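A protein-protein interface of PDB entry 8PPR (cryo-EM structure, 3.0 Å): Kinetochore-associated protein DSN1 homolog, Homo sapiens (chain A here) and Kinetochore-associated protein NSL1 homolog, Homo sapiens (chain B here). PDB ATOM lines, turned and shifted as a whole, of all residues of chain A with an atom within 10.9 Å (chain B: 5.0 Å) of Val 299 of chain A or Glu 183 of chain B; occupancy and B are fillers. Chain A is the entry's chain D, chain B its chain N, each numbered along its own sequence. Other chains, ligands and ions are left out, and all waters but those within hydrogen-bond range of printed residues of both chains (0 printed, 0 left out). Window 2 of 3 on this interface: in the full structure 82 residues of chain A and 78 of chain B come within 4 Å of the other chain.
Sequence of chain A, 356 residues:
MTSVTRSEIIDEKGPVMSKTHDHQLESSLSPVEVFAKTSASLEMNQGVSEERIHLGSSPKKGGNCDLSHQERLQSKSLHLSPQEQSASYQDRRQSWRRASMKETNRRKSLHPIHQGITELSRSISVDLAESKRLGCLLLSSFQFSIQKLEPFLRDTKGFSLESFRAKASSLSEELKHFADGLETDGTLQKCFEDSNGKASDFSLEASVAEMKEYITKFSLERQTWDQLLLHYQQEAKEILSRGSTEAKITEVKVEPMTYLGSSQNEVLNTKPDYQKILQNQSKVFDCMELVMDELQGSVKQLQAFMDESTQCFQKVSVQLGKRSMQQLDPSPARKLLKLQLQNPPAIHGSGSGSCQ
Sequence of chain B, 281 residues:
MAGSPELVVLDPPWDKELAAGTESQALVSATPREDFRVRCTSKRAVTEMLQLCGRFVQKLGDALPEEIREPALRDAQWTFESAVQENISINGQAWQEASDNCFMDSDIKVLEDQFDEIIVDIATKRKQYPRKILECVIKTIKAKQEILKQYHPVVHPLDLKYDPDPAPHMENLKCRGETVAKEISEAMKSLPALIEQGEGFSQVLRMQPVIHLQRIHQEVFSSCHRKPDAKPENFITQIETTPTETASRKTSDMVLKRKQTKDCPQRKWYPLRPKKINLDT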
ATOM      1  N   VAL A 291      12.785   8.045  38.308  1.00  0.00           N
ATOM      2  CA  VAL A 291      12.089   6.791  38.033  1.00  0.00           C
ATOM      3  C   VAL A 291      11.761   6.692  36.554  1.00  0.00           C
ATOM      4  O   VAL A 291      11.831   5.614  35.948  1.00  0.00           O
ATOM      5  CB  VAL A 291      10.821   6.684  38.901  1.00  0.00           C
ATOM      6  CG1 VAL A 291       9.906   5.585  38.378  1.00  0.00           C
ATOM      7  CG2 VAL A 291      11.192   6.435  40.353  1.00  0.00           C
ATOM      8  N   MET A 292      11.397   7.819  35.949  1.00  0.00           N
ATOM      9  CA  MET A 292      11.080   7.833  34.531  1.00  0.00           C
ATOM     10  C   MET A 292      12.299   7.468  33.694  1.00  0.00           C
ATOM     11  O   MET A 292      12.196   6.718  32.712  1.00  0.00           O
ATOM     12  CB  MET A 292      10.561   9.214  34.147  1.00  0.00           C
ATOM     13  CG  MET A 292      10.071   9.223  32.756  1.00  0.00           C
ATOM     14  SD  MET A 292       8.655   8.130  32.812  1.00  0.00           S
ATOM     15  CE  MET A 292       8.615   7.651  31.117  1.00  0.00           C
ATOM     16  N   ASP A 293      13.463   8.000  34.065  1.00  0.00           N
ATOM     17  CA  ASP A 293      14.697   7.642  33.372  1.00  0.00           C
ATOM     18  C   ASP A 293      14.973   6.152  33.500  1.00  0.00           C
ATOM     19  O   ASP A 293      15.375   5.493  32.531  1.00  0.00           O
ATOM     20  CB  ASP A 293      15.866   8.451  33.929  1.00  0.00           C
ATOM     21  CG  ASP A 293      15.667   9.938  33.781  1.00  0.00           C
ATOM     22  OD1 ASP A 293      14.672  10.344  33.144  1.00  0.00           O
ATOM     23  OD2 ASP A 293      16.491  10.701  34.325  1.00  0.00           O
ATOM     24  N   GLU A 294      14.767   5.606  34.701  1.00  0.00           N
ATOM     25  CA  GLU A 294      14.960   4.174  34.907  1.00  0.00           C
ATOM     26  C   GLU A 294      14.035   3.358  34.012  1.00  0.00           C
ATOM     27  O   GLU A 294      14.450   2.349  33.424  1.00  0.00           O
ATOM     28  CB  GLU A 294      14.722   3.823  36.376  1.00  0.00           C
ATOM     29  CG  GLU A 294      15.212   2.441  36.774  1.00  0.00           C
ATOM     30  CD  GLU A 294      15.572   2.352  38.245  1.00  0.00           C
ATOM     31  OE1 GLU A 294      16.128   3.333  38.783  1.00  0.00           O
ATOM     32  OE2 GLU A 294      15.300   1.301  38.865  1.00  0.00           O
ATOM     33  N   LEU A 295      12.774   3.779  33.905  1.00  0.00           N
ATOM     34  CA  LEU A 295      11.820   3.078  33.053  1.00  0.00           C
ATOM     35  C   LEU A 295      12.262   3.105  31.598  1.00  0.00           C
ATOM     36  O   LEU A 295      12.199   2.085  30.897  1.00  0.00           O
ATOM     37  CB  LEU A 295      10.438   3.710  33.196  1.00  0.00           C
ATOM     38  CG  LEU A 295       9.494   3.087  34.220  1.00  0.00           C
ATOM     39  CD1 LEU A 295       8.370   4.051  34.566  1.00  0.00           C
ATOM     40  CD2 LEU A 295       8.943   1.770  33.704  1.00  0.00           C
ATOM     41  N   GLN A 296      12.707   4.271  31.126  1.00  0.00           N
ATOM     42  CA  GLN A 296      13.170   4.377  29.746  1.00  0.00           C
ATOM     43  C   GLN A 296      14.358   3.458  29.497  1.00  0.00           C
ATOM     44  O   GLN A 296      14.428   2.783  28.461  1.00  0.00           O
ATOM     45  CB  GLN A 296      13.535   5.824  29.427  1.00  0.00           C
ATOM     46  CG  GLN A 296      12.380   6.635  28.884  1.00  0.00           C
ATOM     47  CD  GLN A 296      12.833   7.852  28.113  1.00  0.00           C
ATOM     48  OE1 GLN A 296      13.998   8.242  28.172  1.00  0.00           O
ATOM     49  NE2 GLN A 296      11.909   8.466  27.384  1.00  0.00           N
ATOM     50  N   GLY A 297      15.304   3.422  30.437  1.00  0.00           N
ATOM     51  CA  GLY A 297      16.449   2.540  30.284  1.00  0.00           C
ATOM     52  C   GLY A 297      16.054   1.077  30.233  1.00  0.00           C
ATOM     53  O   GLY A 297      16.586   0.304  29.429  1.00  0.00           O
ATOM     54  N   SER A 298      15.116   0.676  31.092  1.00  0.00           N
ATOM     55  CA  SER A 298      14.661  -0.711  31.081  1.00  0.00           C
ATOM     56  C   SER A 298      14.003  -1.062  29.753  1.00  0.00           C
ATOM     57  O   SER A 298      14.241  -2.142  29.195  1.00  0.00           O
ATOM     58  CB  SER A 298      13.699  -0.952  32.242  1.00  0.00           C
ATOM     59  OG  SER A 298      14.409  -1.160  33.450  1.00  0.00           O
ATOM     60  N   VAL A 299      13.176  -0.155  29.227  1.00  0.00           N
ATOM     61  CA  VAL A 299      12.519  -0.410  27.949  1.00  0.00           C
ATOM     62  C   VAL A 299      13.549  -0.538  26.836  1.00  0.00           C
ATOM     63  O   VAL A 299      13.442  -1.411  25.964  1.00  0.00           O
ATOM     64  CB  VAL A 299      11.491   0.696  27.647  1.00  0.00           C
ATOM     65  CG1 VAL A 299      10.984   0.575  26.219  1.00  0.00           C
ATOM     66  CG2 VAL A 299      10.338   0.627  28.634  1.00  0.00           C
ATOM     67  N   LYS A 300      14.562   0.331  26.843  1.00  0.00           N
ATOM     68  CA  LYS A 300      15.603   0.258  25.822  1.00  0.00           C
ATOM     69  C   LYS A 300      16.352  -1.066  25.891  1.00  0.00           C
ATOM     70  O   LYS A 300      16.639  -1.688  24.855  1.00  0.00           O
ATOM     71  CB  LYS A 300      16.577   1.422  25.987  1.00  0.00           C
ATOM     72  CG  LYS A 300      17.832   1.302  25.150  1.00  0.00           C
ATOM     73  CD  LYS A 300      19.051   1.665  25.974  1.00  0.00           C
ATOM     74  CE  LYS A 300      19.165   3.166  26.176  1.00  0.00           C
ATOM     75  NZ  LYS A 300      20.480   3.540  26.765  1.00  0.00           N
ATOM     76  N   GLN A 301      16.688  -1.510  27.106  1.00  0.00           N
ATOM     77  CA  GLN A 301      17.379  -2.787  27.252  1.00  0.00           C
ATOM     78  C   GLN A 301      16.528  -3.937  26.728  1.00  0.00           C
ATOM     79  O   GLN A 301      17.028  -4.808  26.006  1.00  0.00           O
ATOM     80  CB  GLN A 301      17.760  -3.015  28.711  1.00  0.00           C
ATOM     81  CG  GLN A 301      18.900  -2.133  29.183  1.00  0.00           C
ATOM     82  CD  GLN A 301      20.186  -2.369  28.405  1.00  0.00           C
ATOM     83  OE1 GLN A 301      20.961  -3.270  28.734  1.00  0.00           O
ATOM     84  NE2 GLN A 301      20.408  -1.579  27.364  1.00  0.00           N
ATOM     85  N   LEU A 302      15.234  -3.945  27.059  1.00  0.00           N
ATOM     86  CA  LEU A 302      14.362  -5.010  26.570  1.00  0.00           C
ATOM     87  C   LEU A 302      14.268  -4.998  25.049  1.00  0.00           C
ATOM     88  O   LEU A 302      14.272  -6.056  24.404  1.00  0.00           O
ATOM     89  CB  LEU A 302      12.974  -4.875  27.189  1.00  0.00           C
ATOM     90  CG  LEU A 302      11.992  -5.982  26.804  1.00  0.00           C
ATOM     91  CD1 LEU A 302      12.523  -7.342  27.233  1.00  0.00           C
ATOM     92  CD2 LEU A 302      10.616  -5.716  27.391  1.00  0.00           C
ATOM     93  N   GLN A 303      14.170  -3.806  24.459  1.00  0.00           N
ATOM     94  CA  GLN A 303      14.101  -3.697  23.006  1.00  0.00           C
ATOM     95  C   GLN A 303      15.347  -4.272  22.356  1.00  0.00           C
ATOM     96  O   GLN A 303      15.254  -5.112  21.446  1.00  0.00           O
ATOM     97  CB  GLN A 303      13.886  -2.236  22.587  1.00  0.00           C
ATOM     98  CG  GLN A 303      12.412  -1.866  22.494  1.00  0.00           C
ATOM     99  CD  GLN A 303      12.156  -0.370  22.550  1.00  0.00           C
ATOM    100  OE1 GLN A 303      13.092   0.433  22.565  1.00  0.00           O
ATOM    101  NE2 GLN A 303      10.884   0.011  22.570  1.00  0.00           N
ATOM    102  N   ALA A 304      16.520  -3.869  22.840  1.00  0.00           N
ATOM    103  CA  ALA A 304      17.751  -4.436  22.308  1.00  0.00           C
ATOM    104  C   ALA A 304      17.776  -5.942  22.501  1.00  0.00           C
ATOM    105  O   ALA A 304      18.290  -6.680  21.648  1.00  0.00           O
ATOM    106  CB  ALA A 304      18.960  -3.785  22.971  1.00  0.00           C
ATOM    107  N   PHE A 305      17.208  -6.422  23.609  1.00  0.00           N
ATOM    108  CA  PHE A 305      17.235  -7.853  23.862  1.00  0.00           C
ATOM    109  C   PHE A 305      16.468  -8.631  22.805  1.00  0.00           C
ATOM    110  O   PHE A 305      17.009  -9.577  22.215  1.00  0.00           O
ATOM    111  CB  PHE A 305      16.676  -8.169  25.241  1.00  0.00           C
ATOM    112  CG  PHE A 305      16.450  -9.628  25.459  1.00  0.00           C
ATOM    113  CD1 PHE A 305      17.515 -10.507  25.476  1.00  0.00           C
ATOM    114  CD2 PHE A 305      15.171 -10.126  25.623  1.00  0.00           C
ATOM    115  CE1 PHE A 305      17.311 -11.855  25.663  1.00  0.00           C
ATOM    116  CE2 PHE A 305      14.961 -11.469  25.813  1.00  0.00           C
ATOM    117  CZ  PHE A 305      16.028 -12.336  25.834  1.00  0.00           C
ATOM    118  N   MET A 306      15.206  -8.273  22.546  1.00  0.00           N
ATOM    119  CA  MET A 306      14.504  -9.141  21.603  1.00  0.00           C
ATOM    120  C   MET A 306      15.000  -8.892  20.187  1.00  0.00           C
ATOM    121  O   MET A 306      14.879  -9.770  19.328  1.00  0.00           O
ATOM    122  CB  MET A 306      12.970  -9.038  21.625  1.00  0.00           C
ATOM    123  CG  MET A 306      12.297  -7.825  21.026  1.00  0.00           C
ATOM    124  SD  MET A 306      12.446  -6.249  21.829  1.00  0.00           S
ATOM    125  CE  MET A 306      11.458  -6.573  23.285  1.00  0.00           C
ATOM    126  N   ASP A 307      15.560  -7.705  19.918  1.00  0.00           N
ATOM    127  CA  ASP A 307      16.201  -7.496  18.623  1.00  0.00           C
ATOM    128  C   ASP A 307      17.348  -8.477  18.421  1.00  0.00           C
ATOM    129  O   ASP A 307      17.472  -9.101  17.355  1.00  0.00           O
ATOM    130  CB  ASP A 307      16.713  -6.060  18.514  1.00  0.00           C
ATOM    131  CG  ASP A 307      15.592  -5.042  18.461  1.00  0.00           C
ATOM    132  OD1 ASP A 307      14.421  -5.433  18.656  1.00  0.00           O
ATOM    133  OD2 ASP A 307      15.881  -3.852  18.223  1.00  0.00           O
ATOM    134  N   GLU A 308      18.191  -8.633  19.444  1.00  0.00           N
ATOM    135  CA  GLU A 308      19.277  -9.604  19.376  1.00  0.00           C
ATOM    136  C   GLU A 308      18.731 -11.015  19.216  1.00  0.00           C
ATOM    137  O   GLU A 308      19.286 -11.827  18.465  1.00  0.00           O
ATOM    138  CB  GLU A 308      20.127  -9.506  20.641  1.00  0.00           C
ATOM    139  CG  GLU A 308      21.007  -8.274  20.710  1.00  0.00           C
ATOM    140  CD  GLU A 308      22.083  -8.396  21.768  1.00  0.00           C
ATOM    141  OE1 GLU A 308      21.995  -9.328  22.596  1.00  0.00           O
ATOM    142  OE2 GLU A 308      23.005  -7.553  21.784  1.00  0.00           O
ATOM    143  N   GLU B 178       3.728   8.993  28.704  1.00  0.00           N
ATOM    144  CA  GLU B 178       2.990   8.532  27.535  1.00  0.00           C
ATOM    145  C   GLU B 178       3.884   7.708  26.619  1.00  0.00           C
ATOM    146  O   GLU B 178       3.494   6.630  26.147  1.00  0.00           O
ATOM    147  CB  GLU B 178       2.429   9.729  26.775  1.00  0.00           C
ATOM    148  CG  GLU B 178       1.949   9.376  25.387  1.00  0.00           C
ATOM    149  CD  GLU B 178       1.837  10.584  24.488  1.00  0.00           C
ATOM    150  OE1 GLU B 178       2.803  11.374  24.433  1.00  0.00           O
ATOM    151  OE2 GLU B 178       0.786  10.743  23.834  1.00  0.00           O
ATOM    152  N   THR B 179       5.094   8.209  26.359  1.00  0.00           N
ATOM    153  CA  THR B 179       6.015   7.496  25.482  1.00  0.00           C
ATOM    154  C   THR B 179       6.287   6.089  26.000  1.00  0.00           C
ATOM    155  O   THR B 179       6.167   5.105  25.259  1.00  0.00           O
ATOM    156  CB  THR B 179       7.324   8.277  25.362  1.00  0.00           C
ATOM    157  OG1 THR B 179       7.130   9.417  24.515  1.00  0.00           O
ATOM    158  CG2 THR B 179       8.420   7.400  24.785  1.00  0.00           C
ATOM    159  N   VAL B 180       6.632   5.976  27.281  1.00  0.00           N
ATOM    160  CA  VAL B 180       7.001   4.675  27.832  1.00  0.00           C
ATOM    161  C   VAL B 180       5.782   3.772  27.971  1.00  0.00           C
ATOM    162  O   VAL B 180       5.884   2.552  27.822  1.00  0.00           O
ATOM    163  CB  VAL B 180       7.764   4.845  29.157  1.00  0.00           C
ATOM    164  CG1 VAL B 180       7.736   3.571  29.979  1.00  0.00           C
ATOM    165  CG2 VAL B 180       9.201   5.184  28.839  1.00  0.00           C
ATOM    166  N   ALA B 181       4.611   4.345  28.256  1.00  0.00           N
ATOM    167  CA  ALA B 181       3.400   3.533  28.284  1.00  0.00           C
ATOM    168  C   ALA B 181       3.148   2.894  26.927  1.00  0.00           C
ATOM    169  O   ALA B 181       2.883   1.687  26.831  1.00  0.00           O
ATOM    170  CB  ALA B 181       2.207   4.392  28.704  1.00  0.00           C
ATOM    171  N   LYS B 182       3.263   3.689  25.861  1.00  0.00           N
ATOM    172  CA  LYS B 182       3.120   3.149  24.516  1.00  0.00           C
ATOM    173  C   LYS B 182       4.164   2.072  24.251  1.00  0.00           C
ATOM    174  O   LYS B 182       3.851   1.002  23.716  1.00  0.00           O
ATOM    175  CB  LYS B 182       3.245   4.279  23.498  1.00  0.00           C
ATOM    176  CG  LYS B 182       2.696   3.960  22.125  1.00  0.00           C
ATOM    177  CD  LYS B 182       2.453   5.242  21.351  1.00  0.00           C
ATOM    178  CE  LYS B 182       3.623   6.201  21.512  1.00  0.00           C
ATOM    179  NZ  LYS B 182       3.228   7.615  21.273  1.00  0.00           N
ATOM    180  N   GLU B 183       5.413   2.341  24.635  1.00  0.00           N
ATOM    181  CA  GLU B 183       6.490   1.394  24.372  1.00  0.00           C
ATOM    182  C   GLU B 183       6.277   0.080  25.115  1.00  0.00           C
ATOM    183  O   GLU B 183       6.530  -0.996  24.566  1.00  0.00           O
ATOM    184  CB  GLU B 183       7.828   2.020  24.753  1.00  0.00           C
ATOM    185  CG  GLU B 183       8.385   2.944  23.689  1.00  0.00           C
ATOM    186  CD  GLU B 183       9.695   3.582  24.096  1.00  0.00           C
ATOM    187  OE1 GLU B 183      10.022   3.558  25.301  1.00  0.00           O
ATOM    188  OE2 GLU B 183      10.404   4.101  23.209  1.00  0.00           O
ATOM    189  N   ILE B 184       5.819   0.148  26.363  1.00  0.00           N
ATOM    190  CA  ILE B 184       5.606  -1.060  27.151  1.00  0.00           C
ATOM    191  C   ILE B 184       4.432  -1.854  26.594  1.00  0.00           C
ATOM    192  O   ILE B 184       4.455  -3.092  26.576  1.00  0.00           O
ATOM    193  CB  ILE B 184       5.409  -0.699  28.634  1.00  0.00           C
ATOM    194  CG1 ILE B 184       6.723  -0.193  29.230  1.00  0.00           C
ATOM    195  CG2 ILE B 184       4.957  -1.907  29.426  1.00  0.00           C
ATOM    196  CD1 ILE B 184       6.661   0.062  30.720  1.00  0.00           C
ATOM    197  N   SER B 185       3.388  -1.162  26.129  1.00  0.00           N
ATOM    198  CA  SER B 185       2.296  -1.868  25.466  1.00  0.00           C
ATOM    199  C   SER B 185       2.789  -2.589  24.215  1.00  0.00           C
ATOM    200  O   SER B 185       2.457  -3.762  23.987  1.00  0.00           O
ATOM    201  CB  SER B 185       1.172  -0.889  25.129  1.00  0.00           C
ATOM    202  OG  SER B 185       1.439  -0.197  23.922  1.00  0.00           O
ATOM    203  N   GLU B 186       3.613  -1.916  23.409  1.00  0.00           N
ATOM    204  CA  GLU B 186       4.166  -2.573  22.226  1.00  0.00           C
ATOM    205  C   GLU B 186       5.036  -3.761  22.612  1.00  0.00           C
ATOM    206  O   GLU B 186       5.013  -4.799  21.942  1.00  0.00           O
ATOM    207  CB  GLU B 186       4.976  -1.584  21.386  1.00  0.00           C
ATOM    208  CG  GLU B 186       4.257  -0.298  21.011  1.00  0.00           C
ATOM    209  CD  GLU B 186       3.083  -0.495  20.070  1.00  0.00           C
ATOM    210  OE1 GLU B 186       2.774  -1.646  19.695  1.00  0.00           O
ATOM    211  OE2 GLU B 186       2.458   0.522  19.706  1.00  0.00           O
ATOM    212  N   ALA B 187       5.825  -3.620  23.677  1.00  0.00           N
ATOM    213  CA  ALA B 187       6.707  -4.703  24.095  1.00  0.00           C
ATOM    214  C   ALA B 187       5.918  -5.916  24.566  1.00  0.00           C
ATOM    215  O   ALA B 187       6.252  -7.053  24.216  1.00  0.00           O
ATOM    216  CB  ALA B 187       7.650  -4.218  25.195  1.00  0.00           C
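Hydrophobic or aromatic side chains of chain B within 4 Å of the printed part of chain A: Val 180, Ile 184 and Ala 187. Hydrophobic or aromatic side chains of chain A that line the printed part of chain B: Met 292, Val 299 and Leu 302. Along chain A the printed residues that touch a printed residue of chain B span positions 292 to 302. Among the printed residues, 5 pairs touch across the chains. Among the printed residues, no Asp or Glu carboxylate lies within 4 Å of a Lys or Arg side-chain nitrogen of the other chain.
Val 299 of chain A touches two residues of chain B. Printed residues of chain A within 4 Å of Glu 183 of chain B: Val 299. No residue of chain A comes within 4 Å of Thr 179 of chain B. Of chain A, only Met 292 (3.4 Å) and Gln 296 (3.5 Å) come within 4 Å of Val 180 of chain B. No residue of chain A comes within 4 Å of Ala 181 of chain B. No residue of chain A comes within 4 Å of Lys 182 of chain B. Of chain A, only Val 299 comes within 4 Å of Ile 184 of chain B. Printed residues of chain B within 4 Å of Gln 296 of chain A: Val 180 (3.5 Å). Of the printed residues of chain B, Met 292 of chain A touches Val 180 (3.4 Å). Asp 307 of chain A touches none of the printed residues of chain B. Gly 297 of chain A touches none of the printed residues of chain B.
Among the printed residues, merely in contact across the chains: Met 292 of chain A with Val 180 of chain B, Gln 296 of chain A with Val 180 of chain B, Val 299 of chain A with Glu 183 of chain B, Val 299 of chain A with Ile 184 of chain B and Leu 302 of chain A with Ala 187 of chain B.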
